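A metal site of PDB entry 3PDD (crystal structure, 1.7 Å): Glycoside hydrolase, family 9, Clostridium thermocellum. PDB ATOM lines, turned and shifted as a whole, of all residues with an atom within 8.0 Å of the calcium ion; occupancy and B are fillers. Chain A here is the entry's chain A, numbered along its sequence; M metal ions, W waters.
The calcium ion is bound by water W2 (2.4 Å).
The calcium ion is bound by water W3 (2.4 Å).
The calcium ion is bound by O of Pro 50 (2.4 Å).
O of Thr 48 binds the calcium ion (2.4 Å).
OD2 of Asp 46 is bound to the calcium ion, at 2.4 Å.
Water W1 binds the calcium ion (2.4 Å).
The calcium ion is bound by the side-chain carboxylate (OD1) of Asp 46.
OG1 of Thr 48 binds the calcium ion, at 2.6 Å.
Within 4 Å of the calcium ion: Asp 46, Thr 48 and Pro 50.
The backbone NH of Thr 52 sits close to the side-chain carboxylate of Asp 46 (2.8 Å).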
ATOM      1  N   PHE A  36      -1.054 -13.659 -16.302  1.00  0.00           N
ATOM      2  CA  PHE A  36       0.102 -13.810 -15.489  1.00  0.00           C
ATOM      3  C   PHE A  36       1.112 -14.737 -16.169  1.00  0.00           C
ATOM      4  O   PHE A  36       0.732 -15.827 -16.616  1.00  0.00           O
ATOM      5  CB  PHE A  36      -0.270 -14.397 -14.094  1.00  0.00           C
ATOM      6  CG  PHE A  36      -1.076 -13.457 -13.223  1.00  0.00           C
ATOM      7  CD1 PHE A  36      -0.458 -12.594 -12.382  1.00  0.00           C
ATOM      8  CD2 PHE A  36      -2.451 -13.389 -13.354  1.00  0.00           C
ATOM      9  CE1 PHE A  36      -1.223 -11.718 -11.564  1.00  0.00           C
ATOM     10  CE2 PHE A  36      -3.175 -12.548 -12.590  1.00  0.00           C
ATOM     11  CZ  PHE A  36      -2.554 -11.687 -11.696  1.00  0.00           C
ATOM     12  N   SER A  45      -4.986 -16.693 -16.500  1.00  0.00           N
ATOM     13  CA  SER A  45      -5.619 -15.388 -16.714  1.00  0.00           C
ATOM     14  C   SER A  45      -6.841 -15.165 -15.894  1.00  0.00           C
ATOM     15  O   SER A  45      -7.585 -16.086 -15.593  1.00  0.00           O
ATOM     16  CB  SER A  45      -5.873 -15.096 -18.161  1.00  0.00           C
ATOM     17  OG  SER A  45      -6.878 -15.825 -18.713  1.00  0.00           O
ATOM     18  N   ASP A  46      -7.080 -13.918 -15.551  1.00  0.00           N
ATOM     19  CA  ASP A  46      -8.085 -13.594 -14.499  1.00  0.00           C
ATOM     20  C   ASP A  46      -8.901 -12.402 -14.979  1.00  0.00           C
ATOM     21  O   ASP A  46      -8.414 -11.307 -15.126  1.00  0.00           O
ATOM     22  CB  ASP A  46      -7.426 -13.344 -13.139  1.00  0.00           C
ATOM     23  CG  ASP A  46      -8.381 -13.197 -12.046  1.00  0.00           C
ATOM     24  OD1 ASP A  46      -9.646 -13.158 -12.303  1.00  0.00           O
ATOM     25  OD2 ASP A  46      -7.931 -13.097 -10.824  1.00  0.00           O
ATOM     26  N   THR A  47     -10.161 -12.674 -15.302  1.00  0.00           N
ATOM     27  CA  THR A  47     -11.107 -11.609 -15.675  1.00  0.00           C
ATOM     28  C   THR A  47     -11.668 -10.700 -14.608  1.00  0.00           C
ATOM     29  O   THR A  47     -12.314  -9.681 -14.928  1.00  0.00           O
ATOM     30  CB  THR A  47     -12.294 -12.152 -16.490  1.00  0.00           C
ATOM     31  OG1 THR A  47     -13.090 -12.975 -15.625  1.00  0.00           O
ATOM     32  CG2 THR A  47     -11.828 -12.945 -17.677  1.00  0.00           C
ATOM     33  N   THR A  48     -11.474 -11.025 -13.326  1.00  0.00           N
ATOM     34  CA  THR A  48     -12.031 -10.279 -12.244  1.00  0.00           C
ATOM     35  C   THR A  48     -11.002  -9.735 -11.255  1.00  0.00           C
ATOM     36  O   THR A  48     -10.094 -10.459 -10.813  1.00  0.00           O
ATOM     37  CB  THR A  48     -13.028 -11.164 -11.389  1.00  0.00           C
ATOM     38  OG1 THR A  48     -12.368 -12.377 -10.991  1.00  0.00           O
ATOM     39  CG2 THR A  48     -14.336 -11.567 -12.213  1.00  0.00           C
ATOM     40  N   ALA A  49     -11.225  -8.485 -10.856  1.00  0.00           N
ATOM     41  CA  ALA A  49     -10.515  -7.912  -9.687  1.00  0.00           C
ATOM     42  C   ALA A  49     -11.127  -8.563  -8.431  1.00  0.00           C
ATOM     43  O   ALA A  49     -12.336  -8.695  -8.312  1.00  0.00           O
ATOM     44  CB  ALA A  49     -10.607  -6.421  -9.658  1.00  0.00           C
ATOM     45  N   PRO A  50     -10.300  -8.977  -7.461  1.00  0.00           N
ATOM     46  CA  PRO A  50      -8.852  -8.911  -7.464  1.00  0.00           C
ATOM     47  C   PRO A  50      -8.201  -9.946  -8.376  1.00  0.00           C
ATOM     48  O   PRO A  50      -8.682 -11.073  -8.548  1.00  0.00           O
ATOM     49  CB  PRO A  50      -8.464  -9.138  -6.012  1.00  0.00           C
ATOM     50  CG  PRO A  50      -9.693  -9.718  -5.387  1.00  0.00           C
ATOM     51  CD  PRO A  50     -10.829  -9.660  -6.288  1.00  0.00           C
ATOM     52  N   TYR A  51      -7.171  -9.461  -9.067  1.00  0.00           N
ATOM     53  CA  TYR A  51      -6.420 -10.214 -10.046  1.00  0.00           C
ATOM     54  C   TYR A  51      -5.326 -11.073  -9.403  1.00  0.00           C
ATOM     55  O   TYR A  51      -4.454 -10.527  -8.739  1.00  0.00           O
ATOM     56  CB  TYR A  51      -5.776  -9.264 -11.088  1.00  0.00           C
ATOM     57  CG  TYR A  51      -6.822  -8.473 -11.834  1.00  0.00           C
ATOM     58  CD1 TYR A  51      -7.749  -9.111 -12.710  1.00  0.00           C
ATOM     59  CD2 TYR A  51      -6.951  -7.130 -11.634  1.00  0.00           C
ATOM     60  CE1 TYR A  51      -8.740  -8.351 -13.369  1.00  0.00           C
ATOM     61  CE2 TYR A  51      -7.957  -6.384 -12.305  1.00  0.00           C
ATOM     62  CZ  TYR A  51      -8.826  -6.992 -13.127  1.00  0.00           C
ATOM     63  OH  TYR A  51      -9.814  -6.235 -13.732  1.00  0.00           O
ATOM     64  N   THR A  52      -5.515 -12.406  -9.480  1.00  0.00           N
ATOM     65  CA  THR A  52      -4.652 -13.341  -8.786  1.00  0.00           C
ATOM     66  C   THR A  52      -4.268 -14.497  -9.677  1.00  0.00           C
ATOM     67  O   THR A  52      -5.024 -14.896 -10.564  1.00  0.00           O
ATOM     68  CB  THR A  52      -5.284 -13.897  -7.512  1.00  0.00           C
ATOM     69  OG1 THR A  52      -6.452 -14.639  -7.784  1.00  0.00           O
ATOM     70  CG2 THR A  52      -5.604 -12.785  -6.413  1.00  0.00           C
ATOM     71  N   ALA A  53      -3.139 -15.113  -9.350  1.00  0.00           N
ATOM     72  CA  ALA A  53      -2.695 -16.383  -9.957  1.00  0.00           C
ATOM     73  C   ALA A  53      -1.950 -17.172  -8.919  1.00  0.00           C
ATOM     74  O   ALA A  53      -1.459 -16.578  -7.970  1.00  0.00           O
ATOM     75  CB  ALA A  53      -1.800 -16.168 -11.157  1.00  0.00           C
HETATM   76 CA    CA M   1     -10.054 -12.628  -9.768  1.00  0.00          CA
HETATM   77  O   HOH W   1     -10.966 -14.868 -10.065  1.00  0.00           O
HETATM   78  O   HOH W   2     -11.779 -12.389  -8.169  1.00  0.00           O
HETATM   79  O   HOH W   3      -9.069 -13.964  -8.073  1.00  0.00           O
